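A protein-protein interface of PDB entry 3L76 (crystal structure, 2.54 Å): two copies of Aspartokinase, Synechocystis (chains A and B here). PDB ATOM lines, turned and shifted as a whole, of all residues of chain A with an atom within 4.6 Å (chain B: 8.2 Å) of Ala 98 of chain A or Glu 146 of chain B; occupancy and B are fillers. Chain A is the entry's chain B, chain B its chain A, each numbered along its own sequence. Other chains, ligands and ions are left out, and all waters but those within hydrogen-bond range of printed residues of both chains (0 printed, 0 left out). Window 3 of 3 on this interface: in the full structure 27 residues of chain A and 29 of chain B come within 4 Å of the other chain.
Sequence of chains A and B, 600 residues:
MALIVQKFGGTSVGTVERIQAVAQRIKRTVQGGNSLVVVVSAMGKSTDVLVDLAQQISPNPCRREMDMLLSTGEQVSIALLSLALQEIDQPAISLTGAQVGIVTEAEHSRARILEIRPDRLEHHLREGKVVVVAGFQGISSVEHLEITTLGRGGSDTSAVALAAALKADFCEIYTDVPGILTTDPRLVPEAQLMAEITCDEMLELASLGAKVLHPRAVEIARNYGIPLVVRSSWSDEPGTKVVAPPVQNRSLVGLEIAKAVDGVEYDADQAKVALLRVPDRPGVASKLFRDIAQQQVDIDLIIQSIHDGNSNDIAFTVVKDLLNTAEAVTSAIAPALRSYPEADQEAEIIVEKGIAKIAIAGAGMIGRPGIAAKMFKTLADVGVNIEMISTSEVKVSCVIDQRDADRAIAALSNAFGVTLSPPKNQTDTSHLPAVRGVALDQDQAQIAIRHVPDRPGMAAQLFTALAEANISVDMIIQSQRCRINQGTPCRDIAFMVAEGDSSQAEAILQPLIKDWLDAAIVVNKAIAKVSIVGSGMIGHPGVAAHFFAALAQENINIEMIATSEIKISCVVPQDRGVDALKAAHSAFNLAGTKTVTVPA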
ATOM      1  N   THR A  96      11.067 -28.617  -7.089  1.00  0.00           N
ATOM      2  CA  THR A  96      11.163 -28.993  -5.687  1.00  0.00           C
ATOM      3  C   THR A  96       9.767 -29.125  -5.063  1.00  0.00           C
ATOM      4  O   THR A  96       8.790 -28.566  -5.579  1.00  0.00           O
ATOM      5  CB  THR A  96      12.005 -27.941  -4.910  1.00  0.00           C
ATOM      6  OG1 THR A  96      13.144 -28.567  -4.302  1.00  0.00           O
ATOM      7  CG2 THR A  96      11.168 -27.251  -3.844  1.00  0.00           C
ATOM      8  N   GLY A  97       9.673 -29.880  -3.973  1.00  0.00           N
ATOM      9  CA  GLY A  97       8.448 -29.947  -3.201  1.00  0.00           C
ATOM     10  C   GLY A  97       7.149 -30.052  -3.990  1.00  0.00           C
ATOM     11  O   GLY A  97       7.003 -30.903  -4.870  1.00  0.00           O
ATOM     12  N   ALA A  98       6.198 -29.179  -3.669  1.00  0.00           N
ATOM     13  CA  ALA A  98       4.844 -29.269  -4.206  1.00  0.00           C
ATOM     14  C   ALA A  98       4.768 -29.118  -5.726  1.00  0.00           C
ATOM     15  O   ALA A  98       3.717 -29.341  -6.320  1.00  0.00           O
ATOM     16  CB  ALA A  98       3.950 -28.253  -3.533  1.00  0.00           C
ATOM     17  N   GLN A  99       5.876 -28.736  -6.352  1.00  0.00           N
ATOM     18  CA  GLN A  99       5.934 -28.638  -7.809  1.00  0.00           C
ATOM     19  C   GLN A  99       6.056 -30.025  -8.455  1.00  0.00           C
ATOM     20  O   GLN A  99       5.748 -30.214  -9.636  1.00  0.00           O
ATOM     21  CB  GLN A  99       7.101 -27.743  -8.242  1.00  0.00           C
ATOM     22  CG  GLN A  99       6.985 -26.293  -7.789  1.00  0.00           C
ATOM     23  CD  GLN A  99       8.253 -25.500  -8.044  1.00  0.00           C
ATOM     24  OE1 GLN A  99       9.361 -25.959  -7.748  1.00  0.00           O
ATOM     25  NE2 GLN A  99       8.096 -24.298  -8.592  1.00  0.00           N
ATOM     26  N   VAL A 100       6.503 -30.996  -7.666  1.00  0.00           N
ATOM     27  CA  VAL A 100       6.721 -32.348  -8.161  1.00  0.00           C
ATOM     28  C   VAL A 100       5.673 -33.325  -7.631  1.00  0.00           C
ATOM     29  O   VAL A 100       5.201 -34.197  -8.358  1.00  0.00           O
ATOM     30  CB  VAL A 100       8.103 -32.866  -7.756  1.00  0.00           C
ATOM     31  CG1 VAL A 100       8.358 -34.227  -8.384  1.00  0.00           C
ATOM     32  CG2 VAL A 100       9.185 -31.860  -8.154  1.00  0.00           C
ATOM     33  N   GLY A 101       5.312 -33.185  -6.362  1.00  0.00           N
ATOM     34  CA  GLY A 101       4.344 -34.087  -5.777  1.00  0.00           C
ATOM     35  C   GLY A 101       4.122 -33.933  -4.288  1.00  0.00           C
ATOM     36  O   GLY A 101       4.676 -33.048  -3.643  1.00  0.00           O
ATOM     37  N   ASP A 119       2.625 -34.780  -9.880  1.00  0.00           N
ATOM     38  CA  ASP A 119       1.687 -34.049 -10.737  1.00  0.00           C
ATOM     39  C   ASP A 119       2.197 -33.839 -12.181  1.00  0.00           C
ATOM     40  O   ASP A 119       2.354 -34.815 -12.918  1.00  0.00           O
ATOM     41  CB  ASP A 119       1.216 -32.739 -10.082  1.00  0.00           C
ATOM     42  CG  ASP A 119       2.334 -31.728  -9.906  1.00  0.00           C
ATOM     43  OD1 ASP A 119       3.466 -32.144  -9.576  1.00  0.00           O
ATOM     44  OD2 ASP A 119       2.077 -30.515 -10.092  1.00  0.00           O
ATOM     45  N   PHE A 136       9.372 -33.560  -2.236  1.00  0.00           N
ATOM     46  CA  PHE A 136       7.931 -33.482  -2.391  1.00  0.00           C
ATOM     47  C   PHE A 136       7.440 -32.667  -1.217  1.00  0.00           C
ATOM     48  O   PHE A 136       8.179 -32.446  -0.260  1.00  0.00           O
ATOM     49  CB  PHE A 136       7.297 -34.873  -2.352  1.00  0.00           C
ATOM     50  CG  PHE A 136       7.870 -35.828  -3.355  1.00  0.00           C
ATOM     51  CD1 PHE A 136       7.397 -35.855  -4.660  1.00  0.00           C
ATOM     52  CD2 PHE A 136       8.880 -36.702  -2.996  1.00  0.00           C
ATOM     53  CE1 PHE A 136       7.923 -36.738  -5.587  1.00  0.00           C
ATOM     54  CE2 PHE A 136       9.406 -37.584  -3.918  1.00  0.00           C
ATOM     55  CZ  PHE A 136       8.926 -37.601  -5.216  1.00  0.00           C
ATOM     56  N   GLN A 137       6.201 -32.207  -1.292  1.00  0.00           N
ATOM     57  CA  GLN A 137       5.574 -31.580  -0.141  1.00  0.00           C
ATOM     58  C   GLN A 137       4.974 -32.676   0.757  1.00  0.00           C
ATOM     59  O   GLN A 137       4.353 -33.618   0.261  1.00  0.00           O
ATOM     60  CB  GLN A 137       4.502 -30.596  -0.606  1.00  0.00           C
ATOM     61  CG  GLN A 137       3.784 -29.872   0.509  1.00  0.00           C
ATOM     62  CD  GLN A 137       2.706 -28.962  -0.019  1.00  0.00           C
ATOM     63  OE1 GLN A 137       1.823 -29.396  -0.760  1.00  0.00           O
ATOM     64  NE2 GLN A 137       2.775 -27.687   0.350  1.00  0.00           N
ATOM     65  N   GLU A 146       7.328 -28.096   3.697  1.00  0.00           N
ATOM     66  CA  GLU A 146       7.401 -27.634   2.312  1.00  0.00           C
ATOM     67  C   GLU A 146       8.295 -28.474   1.391  1.00  0.00           C
ATOM     68  O   GLU A 146       8.023 -28.573   0.194  1.00  0.00           O
ATOM     69  CB  GLU A 146       7.857 -26.172   2.273  1.00  0.00           C
ATOM     70  CG  GLU A 146       6.861 -25.185   2.882  1.00  0.00           C
ATOM     71  CD  GLU A 146       5.619 -24.985   2.024  1.00  0.00           C
ATOM     72  OE1 GLU A 146       5.580 -25.507   0.892  1.00  0.00           O
ATOM     73  OE2 GLU A 146       4.681 -24.298   2.484  1.00  0.00           O
ATOM     74  N   ARG B  64      18.388 -17.806 -10.429  1.00  0.00           N
ATOM     75  CA  ARG B  64      17.310 -18.633  -9.893  1.00  0.00           C
ATOM     76  C   ARG B  64      17.918 -19.806  -9.135  1.00  0.00           C
ATOM     77  O   ARG B  64      17.635 -20.025  -7.952  1.00  0.00           O
ATOM     78  CB  ARG B  64      16.401 -19.149 -11.011  1.00  0.00           C
ATOM     79  CG  ARG B  64      15.049 -19.650 -10.517  1.00  0.00           C
ATOM     80  CD  ARG B  64      14.191 -20.239 -11.635  1.00  0.00           C
ATOM     81  NE  ARG B  64      14.353 -21.687 -11.750  1.00  0.00           N
ATOM     82  CZ  ARG B  64      13.645 -22.586 -11.066  1.00  0.00           C
ATOM     83  NH1 ARG B  64      12.710 -22.199 -10.203  1.00  0.00           N
ATOM     84  NH2 ARG B  64      13.879 -23.877 -11.241  1.00  0.00           N
ATOM     85  N   MET B  68      17.975 -20.643  -4.741  1.00  0.00           N
ATOM     86  CA  MET B  68      17.719 -21.964  -4.177  1.00  0.00           C
ATOM     87  C   MET B  68      18.952 -22.463  -3.429  1.00  0.00           C
ATOM     88  O   MET B  68      18.896 -22.766  -2.233  1.00  0.00           O
ATOM     89  CB  MET B  68      17.341 -22.971  -5.276  1.00  0.00           C
ATOM     90  CG  MET B  68      17.257 -24.431  -4.783  1.00  0.00           C
ATOM     91  SD  MET B  68      16.796 -25.642  -6.054  1.00  0.00           S
ATOM     92  CE  MET B  68      17.699 -24.982  -7.462  1.00  0.00           C
ATOM     93  N   SER B  71      19.697 -20.643  -0.389  1.00  0.00           N
ATOM     94  CA  SER B  71      18.615 -20.871   0.565  1.00  0.00           C
ATOM     95  C   SER B  71      18.839 -22.081   1.466  1.00  0.00           C
ATOM     96  O   SER B  71      18.283 -22.142   2.562  1.00  0.00           O
ATOM     97  CB  SER B  71      17.286 -21.045  -0.170  1.00  0.00           C
ATOM     98  OG  SER B  71      16.429 -21.904   0.559  1.00  0.00           O
ATOM     99  N   GLN B  75      18.140 -22.991   5.588  1.00  0.00           N
ATOM    100  CA  GLN B  75      17.274 -24.076   6.024  1.00  0.00           C
ATOM    101  C   GLN B  75      17.928 -24.952   7.075  1.00  0.00           C
ATOM    102  O   GLN B  75      17.257 -25.331   8.035  1.00  0.00           O
ATOM    103  CB  GLN B  75      16.811 -24.934   4.857  1.00  0.00           C
ATOM    104  CG  GLN B  75      15.753 -24.300   4.008  1.00  0.00           C
ATOM    105  CD  GLN B  75      15.552 -25.062   2.725  1.00  0.00           C
ATOM    106  OE1 GLN B  75      15.032 -26.183   2.736  1.00  0.00           O
ATOM    107  NE2 GLN B  75      15.977 -24.470   1.606  1.00  0.00           N
ATOM    108  N   THR B  96       9.068 -22.059   6.649  1.00  0.00           N
ATOM    109  CA  THR B  96       9.831 -21.949   5.412  1.00  0.00           C
ATOM    110  C   THR B  96       8.927 -21.493   4.268  1.00  0.00           C
ATOM    111  O   THR B  96       7.705 -21.669   4.321  1.00  0.00           O
ATOM    112  CB  THR B  96      10.468 -23.314   5.041  1.00  0.00           C
ATOM    113  OG1 THR B  96      11.893 -23.198   4.980  1.00  0.00           O
ATOM    114  CG2 THR B  96       9.937 -23.820   3.709  1.00  0.00           C
ATOM    115  N   GLY B  97       9.532 -20.892   3.243  1.00  0.00           N
ATOM    116  CA  GLY B  97       8.830 -20.542   2.017  1.00  0.00           C
ATOM    117  C   GLY B  97       7.441 -19.956   2.195  1.00  0.00           C
ATOM    118  O   GLY B  97       7.250 -19.015   2.956  1.00  0.00           O
ATOM    119  N   ALA B  98       6.464 -20.523   1.494  1.00  0.00           N
ATOM    120  CA  ALA B  98       5.116 -19.948   1.435  1.00  0.00           C
ATOM    121  C   ALA B  98       4.401 -19.838   2.784  1.00  0.00           C
ATOM    122  O   ALA B  98       3.347 -19.206   2.884  1.00  0.00           O
ATOM    123  CB  ALA B  98       4.254 -20.716   0.441  1.00  0.00           C
ATOM    124  N   GLN B  99       4.968 -20.449   3.817  1.00  0.00           N
ATOM    125  CA  GLN B  99       4.388 -20.364   5.149  1.00  0.00           C
ATOM    126  C   GLN B  99       4.712 -19.026   5.802  1.00  0.00           C
ATOM    127  O   GLN B  99       4.035 -18.602   6.741  1.00  0.00           O
ATOM    128  CB  GLN B  99       4.894 -21.514   6.021  1.00  0.00           C
ATOM    129  CG  GLN B  99       4.477 -22.896   5.530  1.00  0.00           C
ATOM    130  CD  GLN B  99       5.180 -24.023   6.276  1.00  0.00           C
ATOM    131  OE1 GLN B  99       6.406 -24.008   6.449  1.00  0.00           O
ATOM    132  NE2 GLN B  99       4.405 -25.016   6.708  1.00  0.00           N
ATOM    133  N   GLY B 101       6.005 -16.101   3.614  1.00  0.00           N
ATOM    134  CA  GLY B 101       5.718 -15.031   2.681  1.00  0.00           C
ATOM    135  C   GLY B 101       6.067 -15.307   1.234  1.00  0.00           C
ATOM    136  O   GLY B 101       6.486 -16.398   0.873  1.00  0.00           O
ATOM    137  N   ALA B 134      12.815 -19.140   7.776  1.00  0.00           N
ATOM    138  CA  ALA B 134      13.786 -19.095   6.700  1.00  0.00           C
ATOM    139  C   ALA B 134      13.098 -19.360   5.367  1.00  0.00           C
ATOM    140  O   ALA B 134      12.384 -20.358   5.194  1.00  0.00           O
ATOM    141  CB  ALA B 134      14.891 -20.102   6.940  1.00  0.00           C
ATOM    142  N   GLY B 135      13.304 -18.445   4.430  1.00  0.00           N
ATOM    143  CA  GLY B 135      12.787 -18.604   3.089  1.00  0.00           C
ATOM    144  C   GLY B 135      11.433 -17.966   2.836  1.00  0.00           C
ATOM    145  O   GLY B 135      10.611 -17.788   3.738  1.00  0.00           O
ATOM    146  N   PHE B 136      11.217 -17.605   1.579  1.00  0.00           N
ATOM    147  CA  PHE B 136       9.911 -17.191   1.108  1.00  0.00           C
ATOM    148  C   PHE B 136       9.688 -17.949  -0.176  1.00  0.00           C
ATOM    149  O   PHE B 136      10.631 -18.489  -0.753  1.00  0.00           O
ATOM    150  CB  PHE B 136       9.876 -15.690   0.810  1.00  0.00           C
ATOM    151  CG  PHE B 136      10.297 -14.831   1.966  1.00  0.00           C
ATOM    152  CD1 PHE B 136       9.389 -14.481   2.952  1.00  0.00           C
ATOM    153  CD2 PHE B 136      11.601 -14.375   2.065  1.00  0.00           C
ATOM    154  CE1 PHE B 136       9.775 -13.696   4.017  1.00  0.00           C
ATOM    155  CE2 PHE B 136      11.988 -13.593   3.123  1.00  0.00           C
ATOM    156  CZ  PHE B 136      11.074 -13.253   4.101  1.00  0.00           C
ATOM    157  N   GLN B 137       8.445 -17.981  -0.630  1.00  0.00           N
ATOM    158  CA  GLN B 137       8.136 -18.543  -1.933  1.00  0.00           C
ATOM    159  C   GLN B 137       8.356 -17.476  -3.000  1.00  0.00           C
ATOM    160  O   GLN B 137       7.957 -16.333  -2.822  1.00  0.00           O
ATOM    161  CB  GLN B 137       6.694 -19.052  -1.968  1.00  0.00           C
ATOM    162  CG  GLN B 137       6.288 -19.679  -3.284  1.00  0.00           C
ATOM    163  CD  GLN B 137       4.846 -20.130  -3.283  1.00  0.00           C
ATOM    164  OE1 GLN B 137       3.938 -19.341  -3.015  1.00  0.00           O
ATOM    165  NE2 GLN B 137       4.624 -21.409  -3.581  1.00  0.00           N
ATOM    166  N   GLY B 138       9.005 -17.853  -4.097  1.00  0.00           N
ATOM    167  CA  GLY B 138       9.254 -16.950  -5.200  1.00  0.00           C
ATOM    168  C   GLY B 138       8.328 -17.205  -6.370  1.00  0.00           C
ATOM    169  O   GLY B 138       8.137 -18.354  -6.779  1.00  0.00           O
ATOM    170  N   ILE B 139       7.725 -16.121  -6.870  1.00  0.00           N
ATOM    171  CA  ILE B 139       6.845 -16.136  -8.038  1.00  0.00           C
ATOM    172  C   ILE B 139       7.410 -15.262  -9.158  1.00  0.00           C
ATOM    173  O   ILE B 139       7.417 -15.653 -10.328  1.00  0.00           O
ATOM    174  CB  ILE B 139       5.445 -15.670  -7.660  1.00  0.00           C
ATOM    175  N   HIS B 144       8.305 -20.665 -10.982  1.00  0.00           N
ATOM    176  CA  HIS B 144       8.144 -20.464  -9.544  1.00  0.00           C
ATOM    177  C   HIS B 144       9.277 -21.145  -8.770  1.00  0.00           C
ATOM    178  O   HIS B 144       9.975 -22.002  -9.315  1.00  0.00           O
ATOM    179  CB  HIS B 144       6.768 -20.978  -9.073  1.00  0.00           C
ATOM    180  N   LEU B 145       9.464 -20.752  -7.511  1.00  0.00           N
ATOM    181  CA  LEU B 145      10.461 -21.374  -6.634  1.00  0.00           C
ATOM    182  C   LEU B 145       9.886 -21.596  -5.232  1.00  0.00           C
ATOM    183  O   LEU B 145       9.401 -20.652  -4.618  1.00  0.00           O
ATOM    184  CB  LEU B 145      11.740 -20.520  -6.573  1.00  0.00           C
ATOM    185  N   GLU B 146       9.936 -22.833  -4.729  1.00  0.00           N
ATOM    186  CA  GLU B 146       9.319 -23.153  -3.433  1.00  0.00           C
ATOM    187  C   GLU B 146      10.007 -22.489  -2.227  1.00  0.00           C
ATOM    188  O   GLU B 146       9.333 -22.059  -1.291  1.00  0.00           O
ATOM    189  CB  GLU B 146       9.190 -24.674  -3.232  1.00  0.00           C
ATOM    190  CG  GLU B 146       8.231 -25.348  -4.209  1.00  0.00           C
ATOM    191  CD  GLU B 146       6.762 -25.009  -3.954  1.00  0.00           C
ATOM    192  OE1 GLU B 146       6.456 -24.358  -2.928  1.00  0.00           O
ATOM    193  OE2 GLU B 146       5.909 -25.401  -4.783  1.00  0.00           O
ATOM    194  N   ILE B 147      11.338 -22.426  -2.243  1.00  0.00           N
ATOM    195  CA  ILE B 147      12.096 -21.717  -1.207  1.00  0.00           C
ATOM    196  C   ILE B 147      13.307 -20.976  -1.795  1.00  0.00           C
ATOM    197  O   ILE B 147      14.182 -21.576  -2.425  1.00  0.00           O
ATOM    198  CB  ILE B 147      12.593 -22.650  -0.068  1.00  0.00           C
ATOM    199  CG1 ILE B 147      11.549 -23.710   0.285  1.00  0.00           C
ATOM    200  CG2 ILE B 147      12.947 -21.835   1.165  1.00  0.00           C
ATOM    201  CD1 ILE B 147      12.012 -24.682   1.338  1.00  0.00           C
ATOM    202  N   THR B 148      13.346 -19.665  -1.589  1.00  0.00           N
ATOM    203  CA  THR B 148      14.502 -18.865  -1.969  1.00  0.00           C
ATOM    204  C   THR B 148      14.783 -17.802  -0.921  1.00  0.00           C
ATOM    205  O   THR B 148      13.931 -17.483  -0.093  1.00  0.00           O
ATOM    206  CB  THR B 148      14.300 -18.161  -3.318  1.00  0.00           C
ATOM    207  OG1 THR B 148      13.137 -17.321  -3.255  1.00  0.00           O
ATOM    208  CG2 THR B 148      14.140 -19.185  -4.434  1.00  0.00           C
ATOM    209  N   THR B 149      15.986 -17.251  -0.968  1.00  0.00           N
ATOM    210  CA  THR B 149      16.350 -16.167  -0.076  1.00  0.00           C
ATOM    211  C   THR B 149      16.322 -14.849  -0.846  1.00  0.00           C
ATOM    212  O   THR B 149      16.087 -14.837  -2.058  1.00  0.00           O
ATOM    213  CB  THR B 149      17.734 -16.404   0.522  1.00  0.00           C
ATOM    214  OG1 THR B 149      18.694 -16.524  -0.535  1.00  0.00           O
ATOM    215  CG2 THR B 149      17.726 -17.680   1.339  1.00  0.00           C
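Thr 96 of chain A touches Glu 146 of chain B, and with the chains exchanged Glu 146 of chain A touches Thr 96 of chain B.
Ala 98 of chain A touches Glu 146 of chain B, but with the chains exchanged Glu 146 of chain A does not touch Ala 98 of chain B (4.1 Å).
Gln 99 of chain A touches Glu 146 of chain B, and with the chains exchanged Glu 146 of chain A touches Gln 99 of chain B.
Of the printed residues of chain B, Thr 96 of chain A touches Glu 146.
No residue of chain B comes within 4 Å of Gly 97 of chain A.
Ala 98 of chain A touches one residue of chain B.
Printed residues of chain B within 4 Å of Gln 99 of chain A: His 144, Leu 145 and Glu 146.
Of the printed residues of chain A, His 144 of chain B touches Gln 99.
Glu 146 of chain B touches three residues of chain A.
Thr 149 of chain B touches none of the printed residues of chain A.
Among the printed residues, merely in contact across the chains: Thr 96 of chain A with Glu 146 of chain B (3.3 Å), Ala 98 of chain A with Glu 146 of chain B (3.7 Å), Gln 99 of chain A with Leu 145 of chain B (3.95 Å), Gln 99 of chain A with Glu 146 of chain B (3.3 Å), Glu 146 of chain A with Thr 96 of chain B (3.5 Å) and Glu 146 of chain A with Gln 99 of chain B (3.4 Å).
Hydrophobic or aromatic side chains of chain A within 4 Å of the printed part of chain B: Ala 98.
Of the 21 printed residues of chain B, 5 touch a printed residue of chain A.
Hydrophobic or aromatic side chains of chain B within 4 Å of the printed part of chain A: His 144.
Among the printed residues, no Asp or Glu carboxylate lies within 4 Å of a Lys or Arg side-chain nitrogen of the other chain.
The backbone carbonyl oxygen (O) of His 144 of chain B lies within hydrogen-bond range of the side-chain amide nitrogen (NE2) of Gln 99 of chain A, 3.1 Å away.
O of His 144 of chain B is in hydrogen-bond range of NH1 of Arg 64 of chain B (2.9 Å).
N of Thr 96 of chain B sits at hydrogen-bond distance from OE1 of Gln 99 of chain B (3.3 Å).
The backbone carbonyl oxygen (O) of Ala 134 of chain B is in hydrogen-bond range of the side-chain hydroxyl (OG1) of Thr 96 of chain B (2.9 Å).
N of Leu 145 of chain B lies within hydrogen-bond range of O of Gly 138 of chain B.
N of Thr 96 of chain A sits at hydrogen-bond distance from OE1 of Gln 99 of chain A, at 3.2 Å.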
